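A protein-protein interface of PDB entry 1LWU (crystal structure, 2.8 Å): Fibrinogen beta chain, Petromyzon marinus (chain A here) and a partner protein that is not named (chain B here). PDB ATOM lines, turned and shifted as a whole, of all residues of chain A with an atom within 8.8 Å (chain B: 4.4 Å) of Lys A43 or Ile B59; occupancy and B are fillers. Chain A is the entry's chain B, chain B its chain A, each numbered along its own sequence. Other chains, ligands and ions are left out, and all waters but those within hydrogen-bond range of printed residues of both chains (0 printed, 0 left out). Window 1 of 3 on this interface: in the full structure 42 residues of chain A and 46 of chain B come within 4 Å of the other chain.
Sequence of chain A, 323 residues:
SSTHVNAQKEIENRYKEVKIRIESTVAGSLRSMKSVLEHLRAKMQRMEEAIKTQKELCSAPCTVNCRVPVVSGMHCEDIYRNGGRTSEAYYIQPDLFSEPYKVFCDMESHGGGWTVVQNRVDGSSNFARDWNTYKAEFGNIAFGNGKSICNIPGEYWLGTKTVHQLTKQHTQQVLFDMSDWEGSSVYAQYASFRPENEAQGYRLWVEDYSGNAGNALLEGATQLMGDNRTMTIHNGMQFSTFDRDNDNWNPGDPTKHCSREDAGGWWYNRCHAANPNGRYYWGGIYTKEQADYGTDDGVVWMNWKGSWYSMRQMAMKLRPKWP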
ATOM      1  N   SER A  35       2.345  28.161  29.048  1.00  0.00           N
ATOM      2  CA  SER A  35       3.395  27.475  29.782  1.00  0.00           C
ATOM      3  C   SER A  35       4.289  26.774  28.751  1.00  0.00           C
ATOM      4  O   SER A  35       5.509  26.944  28.751  1.00  0.00           O
ATOM      5  CB  SER A  35       2.781  26.461  30.753  1.00  0.00           C
ATOM      6  OG  SER A  35       3.652  26.201  31.842  1.00  0.00           O
ATOM      7  N   VAL A  36       3.669  25.998  27.866  1.00  0.00           N
ATOM      8  CA  VAL A  36       4.405  25.299  26.826  1.00  0.00           C
ATOM      9  C   VAL A  36       5.208  26.313  26.022  1.00  0.00           C
ATOM     10  O   VAL A  36       6.408  26.135  25.812  1.00  0.00           O
ATOM     11  CB  VAL A  36       3.452  24.539  25.880  1.00  0.00           C
ATOM     12  CG1 VAL A  36       4.148  24.216  24.575  1.00  0.00           C
ATOM     13  CG2 VAL A  36       3.000  23.254  26.542  1.00  0.00           C
ATOM     14  N   LEU A  37       4.550  27.375  25.566  1.00  0.00           N
ATOM     15  CA  LEU A  37       5.251  28.402  24.810  1.00  0.00           C
ATOM     16  C   LEU A  37       6.405  28.942  25.640  1.00  0.00           C
ATOM     17  O   LEU A  37       7.485  29.180  25.125  1.00  0.00           O
ATOM     18  CB  LEU A  37       4.300  29.532  24.445  1.00  0.00           C
ATOM     19  CG  LEU A  37       3.303  29.122  23.358  1.00  0.00           C
ATOM     20  CD1 LEU A  37       2.157  30.102  23.280  1.00  0.00           C
ATOM     21  CD2 LEU A  37       4.020  29.047  22.034  1.00  0.00           C
ATOM     22  N   GLU A  38       6.173  29.109  26.935  1.00  0.00           N
ATOM     23  CA  GLU A  38       7.190  29.612  27.850  1.00  0.00           C
ATOM     24  C   GLU A  38       8.290  28.560  28.064  1.00  0.00           C
ATOM     25  O   GLU A  38       9.478  28.885  28.153  1.00  0.00           O
ATOM     26  CB  GLU A  38       6.536  29.955  29.188  1.00  0.00           C
ATOM     27  CG  GLU A  38       7.030  31.240  29.830  1.00  0.00           C
ATOM     28  CD  GLU A  38       6.158  31.667  31.012  1.00  0.00           C
ATOM     29  OE1 GLU A  38       4.914  31.701  30.846  1.00  0.00           O
ATOM     30  OE2 GLU A  38       6.710  31.975  32.094  1.00  0.00           O
ATOM     31  N   HIS A  39       7.881  27.299  28.157  1.00  0.00           N
ATOM     32  CA  HIS A  39       8.810  26.196  28.351  1.00  0.00           C
ATOM     33  C   HIS A  39       9.710  26.109  27.114  1.00  0.00           C
ATOM     34  O   HIS A  39      10.937  26.033  27.210  1.00  0.00           O
ATOM     35  CB  HIS A  39       8.024  24.891  28.530  1.00  0.00           C
ATOM     36  CG  HIS A  39       8.872  23.703  28.872  1.00  0.00           C
ATOM     37  ND1 HIS A  39       9.962  23.319  28.119  1.00  0.00           N
ATOM     38  CD2 HIS A  39       8.768  22.795  29.873  1.00  0.00           C
ATOM     39  CE1 HIS A  39      10.493  22.226  28.639  1.00  0.00           C
ATOM     40  NE2 HIS A  39       9.786  21.886  29.703  1.00  0.00           N
ATOM     41  N   LEU A  40       9.089  26.128  25.944  1.00  0.00           N
ATOM     42  CA  LEU A  40       9.841  26.063  24.700  1.00  0.00           C
ATOM     43  C   LEU A  40      10.934  27.124  24.657  1.00  0.00           C
ATOM     44  O   LEU A  40      12.084  26.827  24.336  1.00  0.00           O
ATOM     45  CB  LEU A  40       8.905  26.249  23.503  1.00  0.00           C
ATOM     46  CG  LEU A  40       7.926  25.118  23.201  1.00  0.00           C
ATOM     47  CD1 LEU A  40       7.163  25.458  21.933  1.00  0.00           C
ATOM     48  CD2 LEU A  40       8.678  23.812  23.037  1.00  0.00           C
ATOM     49  N   ARG A  41      10.572  28.361  24.979  1.00  0.00           N
ATOM     50  CA  ARG A  41      11.533  29.452  24.960  1.00  0.00           C
ATOM     51  C   ARG A  41      12.770  29.087  25.779  1.00  0.00           C
ATOM     52  O   ARG A  41      13.881  29.047  25.253  1.00  0.00           O
ATOM     53  CB  ARG A  41      10.892  30.721  25.505  1.00  0.00           C
ATOM     54  CG  ARG A  41      11.345  31.986  24.806  1.00  0.00           C
ATOM     55  CD  ARG A  41      11.255  33.167  25.747  1.00  0.00           C
ATOM     56  NE  ARG A  41      11.874  32.861  27.040  1.00  0.00           N
ATOM     57  CZ  ARG A  41      11.211  32.445  28.121  1.00  0.00           C
ATOM     58  NH1 ARG A  41       9.894  32.286  28.086  1.00  0.00           N
ATOM     59  NH2 ARG A  41      11.869  32.171  29.238  1.00  0.00           N
ATOM     60  N   ALA A  42      12.577  28.805  27.061  1.00  0.00           N
ATOM     61  CA  ALA A  42      13.685  28.431  27.929  1.00  0.00           C
ATOM     62  C   ALA A  42      14.515  27.283  27.338  1.00  0.00           C
ATOM     63  O   ALA A  42      15.728  27.205  27.549  1.00  0.00           O
ATOM     64  CB  ALA A  42      13.156  28.036  29.296  1.00  0.00           C
ATOM     65  N   LYS A  43      13.867  26.377  26.615  1.00  0.00           N
ATOM     66  CA  LYS A  43      14.602  25.274  26.010  1.00  0.00           C
ATOM     67  C   LYS A  43      15.559  25.893  24.984  1.00  0.00           C
ATOM     68  O   LYS A  43      16.746  25.541  24.935  1.00  0.00           O
ATOM     69  CB  LYS A  43      13.642  24.271  25.332  1.00  0.00           C
ATOM     70  CG  LYS A  43      14.366  23.199  24.526  1.00  0.00           C
ATOM     71  CD  LYS A  43      13.444  22.132  23.979  1.00  0.00           C
ATOM     72  CE  LYS A  43      13.042  21.129  25.070  1.00  0.00           C
ATOM     73  NZ  LYS A  43      14.135  20.187  25.511  1.00  0.00           N
ATOM     74  N   MET A  44      15.041  26.840  24.196  1.00  0.00           N
ATOM     75  CA  MET A  44      15.827  27.514  23.175  1.00  0.00           C
ATOM     76  C   MET A  44      16.986  28.320  23.742  1.00  0.00           C
ATOM     77  O   MET A  44      18.069  28.341  23.157  1.00  0.00           O
ATOM     78  CB  MET A  44      14.936  28.406  22.336  1.00  0.00           C
ATOM     79  CG  MET A  44      13.762  27.646  21.783  1.00  0.00           C
ATOM     80  SD  MET A  44      13.264  28.129  20.132  1.00  0.00           S
ATOM     81  CE  MET A  44      11.894  29.162  20.521  1.00  0.00           C
ATOM     82  N   GLN A  45      16.773  28.991  24.870  1.00  0.00           N
ATOM     83  CA  GLN A  45      17.859  29.747  25.484  1.00  0.00           C
ATOM     84  C   GLN A  45      18.961  28.767  25.888  1.00  0.00           C
ATOM     85  O   GLN A  45      20.107  28.922  25.467  1.00  0.00           O
ATOM     86  CB  GLN A  45      17.364  30.512  26.710  1.00  0.00           C
ATOM     87  CG  GLN A  45      16.464  31.690  26.373  1.00  0.00           C
ATOM     88  CD  GLN A  45      15.748  32.255  27.590  1.00  0.00           C
ATOM     89  OE1 GLN A  45      14.937  33.173  27.472  1.00  0.00           O
ATOM     90  NE2 GLN A  45      16.044  31.705  28.763  1.00  0.00           N
ATOM     91  N   ARG A  46      18.622  27.750  26.685  1.00  0.00           N
ATOM     92  CA  ARG A  46      19.623  26.773  27.114  1.00  0.00           C
ATOM     93  C   ARG A  46      20.433  26.326  25.916  1.00  0.00           C
ATOM     94  O   ARG A  46      21.628  26.035  26.038  1.00  0.00           O
ATOM     95  CB  ARG A  46      18.982  25.544  27.750  1.00  0.00           C
ATOM     96  CG  ARG A  46      18.542  25.730  29.170  1.00  0.00           C
ATOM     97  CD  ARG A  46      18.426  24.388  29.872  1.00  0.00           C
ATOM     98  NE  ARG A  46      17.513  23.438  29.223  1.00  0.00           N
ATOM     99  CZ  ARG A  46      16.189  23.577  29.153  1.00  0.00           C
ATOM    100  NH1 ARG A  46      15.595  24.639  29.689  1.00  0.00           N
ATOM    101  NH2 ARG A  46      15.455  22.637  28.565  1.00  0.00           N
ATOM    102  N   MET A  47      19.764  26.260  24.765  1.00  0.00           N
ATOM    103  CA  MET A  47      20.406  25.870  23.517  1.00  0.00           C
ATOM    104  C   MET A  47      21.233  27.025  22.973  1.00  0.00           C
ATOM    105  O   MET A  47      22.412  26.844  22.663  1.00  0.00           O
ATOM    106  CB  MET A  47      19.371  25.462  22.471  1.00  0.00           C
ATOM    107  CG  MET A  47      19.077  23.983  22.428  1.00  0.00           C
ATOM    108  SD  MET A  47      17.760  23.598  21.287  1.00  0.00           S
ATOM    109  CE  MET A  47      16.403  23.850  22.304  1.00  0.00           C
ATOM    110  N   GLU A  48      20.632  28.209  22.856  1.00  0.00           N
ATOM    111  CA  GLU A  48      21.369  29.354  22.334  1.00  0.00           C
ATOM    112  C   GLU A  48      22.613  29.612  23.163  1.00  0.00           C
ATOM    113  O   GLU A  48      23.662  29.962  22.618  1.00  0.00           O
ATOM    114  CB  GLU A  48      20.514  30.623  22.308  1.00  0.00           C
ATOM    115  CG  GLU A  48      21.140  31.749  21.475  1.00  0.00           C
ATOM    116  CD  GLU A  48      20.179  32.906  21.186  1.00  0.00           C
ATOM    117  OE1 GLU A  48      20.382  33.618  20.183  1.00  0.00           O
ATOM    118  OE2 GLU A  48      19.224  33.118  21.954  1.00  0.00           O
ATOM    119  N   GLU A  49      22.512  29.425  24.474  1.00  0.00           N
ATOM    120  CA  GLU A  49      23.675  29.659  25.311  1.00  0.00           C
ATOM    121  C   GLU A  49      24.691  28.560  25.046  1.00  0.00           C
ATOM    122  O   GLU A  49      25.872  28.847  24.805  1.00  0.00           O
ATOM    123  CB  GLU A  49      23.287  29.720  26.796  1.00  0.00           C
ATOM    124  CG  GLU A  49      23.254  28.392  27.538  1.00  0.00           C
ATOM    125  CD  GLU A  49      24.482  28.179  28.424  1.00  0.00           C
ATOM    126  OE1 GLU A  49      25.603  28.044  27.878  1.00  0.00           O
ATOM    127  OE2 GLU A  49      24.324  28.149  29.669  1.00  0.00           O
ATOM    128  N   ALA A  50      24.239  27.307  25.049  1.00  0.00           N
ATOM    129  CA  ALA A  50      25.149  26.190  24.789  1.00  0.00           C
ATOM    130  C   ALA A  50      25.924  26.380  23.476  1.00  0.00           C
ATOM    131  O   ALA A  50      27.064  25.931  23.367  1.00  0.00           O
ATOM    132  CB  ALA A  50      24.386  24.873  24.765  1.00  0.00           C
ATOM    133  N   GLU A 289      10.857  10.759  15.137  1.00  0.00           N
ATOM    134  CA  GLU A 289      10.536  12.163  15.364  1.00  0.00           C
ATOM    135  C   GLU A 289      11.792  13.033  15.463  1.00  0.00           C
ATOM    136  O   GLU A 289      11.772  14.206  15.107  1.00  0.00           O
ATOM    137  CB  GLU A 289       9.702  12.306  16.645  1.00  0.00           C
ATOM    138  CG  GLU A 289       8.297  11.713  16.569  1.00  0.00           C
ATOM    139  CD  GLU A 289       8.280  10.205  16.341  1.00  0.00           C
ATOM    140  OE1 GLU A 289       8.831   9.456  17.179  1.00  0.00           O
ATOM    141  OE2 GLU A 289       7.706   9.769  15.318  1.00  0.00           O
ATOM    142  N   GLN B  55       5.595  23.428  16.599  1.00  0.00           N
ATOM    143  CA  GLN B  55       6.691  24.275  17.068  1.00  0.00           C
ATOM    144  C   GLN B  55       7.426  23.469  18.123  1.00  0.00           C
ATOM    145  O   GLN B  55       8.622  23.646  18.350  1.00  0.00           O
ATOM    146  CB  GLN B  55       6.187  25.580  17.689  1.00  0.00           C
ATOM    147  CG  GLN B  55       7.322  26.546  17.979  1.00  0.00           C
ATOM    148  CD  GLN B  55       6.886  27.804  18.704  1.00  0.00           C
ATOM    149  OE1 GLN B  55       6.707  27.802  19.923  1.00  0.00           O
ATOM    150  NE2 GLN B  55       6.719  28.892  17.956  1.00  0.00           N
ATOM    151  N   VAL B  56       6.679  22.582  18.770  1.00  0.00           N
ATOM    152  CA  VAL B  56       7.222  21.707  19.797  1.00  0.00           C
ATOM    153  C   VAL B  56       7.984  20.621  19.056  1.00  0.00           C
ATOM    154  O   VAL B  56       8.984  20.092  19.540  1.00  0.00           O
ATOM    155  CB  VAL B  56       6.092  21.050  20.639  1.00  0.00           C
ATOM    156  CG1 VAL B  56       6.689  20.084  21.645  1.00  0.00           C
ATOM    157  CG2 VAL B  56       5.295  22.111  21.362  1.00  0.00           C
ATOM    158  N   SER B  57       7.489  20.297  17.868  1.00  0.00           N
ATOM    159  CA  SER B  57       8.115  19.290  17.027  1.00  0.00           C
ATOM    160  C   SER B  57       9.394  19.873  16.440  1.00  0.00           C
ATOM    161  O   SER B  57      10.464  19.273  16.531  1.00  0.00           O
ATOM    162  CB  SER B  57       7.164  18.887  15.897  1.00  0.00           C
ATOM    163  OG  SER B  57       7.863  18.231  14.854  1.00  0.00           O
ATOM    164  N   GLN B  58       9.267  21.058  15.854  1.00  0.00           N
ATOM    165  CA  GLN B  58      10.393  21.739  15.238  1.00  0.00           C
ATOM    166  C   GLN B  58      11.506  22.004  16.234  1.00  0.00           C
ATOM    167  O   GLN B  58      12.667  21.680  15.973  1.00  0.00           O
ATOM    168  CB  GLN B  58       9.939  23.061  14.630  1.00  0.00           C
ATOM    169  CG  GLN B  58      10.931  23.651  13.661  1.00  0.00           C
ATOM    170  CD  GLN B  58      10.430  24.940  13.050  1.00  0.00           C
ATOM    171  OE1 GLN B  58       9.237  25.079  12.778  1.00  0.00           O
ATOM    172  NE2 GLN B  58      11.336  25.887  12.816  1.00  0.00           N
ATOM    173  N   ILE B  59      11.157  22.592  17.375  1.00  0.00           N
ATOM    174  CA  ILE B  59      12.164  22.885  18.377  1.00  0.00           C
ATOM    175  C   ILE B  59      12.814  21.623  18.900  1.00  0.00           C
ATOM    176  O   ILE B  59      14.003  21.628  19.230  1.00  0.00           O
ATOM    177  CB  ILE B  59      11.587  23.662  19.554  1.00  0.00           C
ATOM    178  CG1 ILE B  59      11.226  25.069  19.093  1.00  0.00           C
ATOM    179  CG2 ILE B  59      12.610  23.737  20.682  1.00  0.00           C
ATOM    180  CD1 ILE B  59      10.655  25.936  20.167  1.00  0.00           C
ATOM    181  N   LEU B  60      12.053  20.535  18.977  1.00  0.00           N
ATOM    182  CA  LEU B  60      12.632  19.299  19.471  1.00  0.00           C
ATOM    183  C   LEU B  60      13.692  18.820  18.503  1.00  0.00           C
ATOM    184  O   LEU B  60      14.821  18.530  18.895  1.00  0.00           O
ATOM    185  CB  LEU B  60      11.578  18.214  19.632  1.00  0.00           C
ATOM    186  CG  LEU B  60      12.199  16.850  19.970  1.00  0.00           C
ATOM    187  CD1 LEU B  60      13.290  17.021  21.063  1.00  0.00           C
ATOM    188  CD2 LEU B  60      11.085  15.870  20.390  1.00  0.00           C
ATOM    189  N   ARG B  61      13.313  18.730  17.235  1.00  0.00           N
ATOM    190  CA  ARG B  61      14.228  18.298  16.191  1.00  0.00           C
ATOM    191  C   ARG B  61      15.504  19.140  16.274  1.00  0.00           C
ATOM    192  O   ARG B  61      16.616  18.607  16.369  1.00  0.00           O
ATOM    193  CB  ARG B  61      13.577  18.479  14.820  1.00  0.00           C
ATOM    194  CG  ARG B  61      14.509  18.187  13.672  1.00  0.00           C
ATOM    195  CD  ARG B  61      14.352  16.772  13.132  1.00  0.00           C
ATOM    196  NE  ARG B  61      13.295  16.711  12.127  1.00  0.00           N
ATOM    197  CZ  ARG B  61      11.997  16.746  12.403  1.00  0.00           C
ATOM    198  NH1 ARG B  61      11.584  16.830  13.660  1.00  0.00           N
ATOM    199  NH2 ARG B  61      11.113  16.718  11.417  1.00  0.00           N
ATOM    200  N   VAL B  62      15.331  20.459  16.255  1.00  0.00           N
ATOM    201  CA  VAL B  62      16.461  21.371  16.321  1.00  0.00           C
ATOM    202  C   VAL B  62      17.393  21.038  17.478  1.00  0.00           C
ATOM    203  O   VAL B  62      18.602  20.966  17.303  1.00  0.00           O
ATOM    204  CB  VAL B  62      16.002  22.824  16.485  1.00  0.00           C
ATOM    205  CG1 VAL B  62      17.184  23.748  16.404  1.00  0.00           C
ATOM    206  CG2 VAL B  62      15.006  23.174  15.413  1.00  0.00           C
ATOM    207  N   GLU B  63      16.839  20.832  18.662  1.00  0.00           N
ATOM    208  CA  GLU B  63      17.677  20.523  19.803  1.00  0.00           C
ATOM    209  C   GLU B  63      18.541  19.291  19.615  1.00  0.00           C
ATOM    210  O   GLU B  63      19.671  19.274  20.070  1.00  0.00           O
ATOM    211  CB  GLU B  63      16.842  20.342  21.066  1.00  0.00           C
ATOM    212  CG  GLU B  63      17.686  20.033  22.289  1.00  0.00           C
ATOM    213  CD  GLU B  63      16.837  19.880  23.520  1.00  0.00           C
ATOM    214  OE1 GLU B  63      15.944  19.005  23.507  1.00  0.00           O
ATOM    215  OE2 GLU B  63      17.051  20.630  24.497  1.00  0.00           O
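Lys A43 touches just these residues of chain B: Ile B59 (3.8 Å) and Glu B63 (2.9 Å). Of the printed residues of chain A, Ile B59 touches Leu A40, Lys A43 and Met A44. Of the printed residues of chain B, Met A44 touches Ile B59. Of the printed residues of chain B, Met A47 touches Glu B63. Printed residues of chain B within 4 Å of Leu A40: Gln B55 (3.1 Å), Val B56 (3.9 Å) and Ile B59 (3.8 Å). Printed residues of chain B within 4 Å of Leu A37: Gln B55. Val B62 touches none of the printed residues of chain A. The nearest printed residue of chain B that does not touch Leu A40 is Leu B60 (6.2 Å).
Among the printed residues, merely in contact across the chains: Leu A37 with Gln B55 (3.6 Å), Leu A40 with Gln B55 (3.1 Å), Leu A40 with Val B56 (3.9 Å), Leu A40 with Ile B59 (3.8 Å), Lys A43 with Ile B59 (3.8 Å), Met A44 with Ile B59 (3.4 Å) and Met A47 with Glu B63 (3.4 Å).
Printed residues of chain A that touch a printed residue of chain B: Leu A37, Leu A40, Lys A43, Met A44, Met A47 and Glu A289. Along chain A the printed residues that touch a printed residue of chain B span positions 37 to 289. Among the printed residues, 9 pairs touch across the chains.
O of Glu A289 sits at hydrogen-bond distance from NH1 of Arg B61. The side-chain amino group of Lys A43 lies within salt-bridge range of the side-chain carboxylate of Glu B63, at 2.9 Å.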
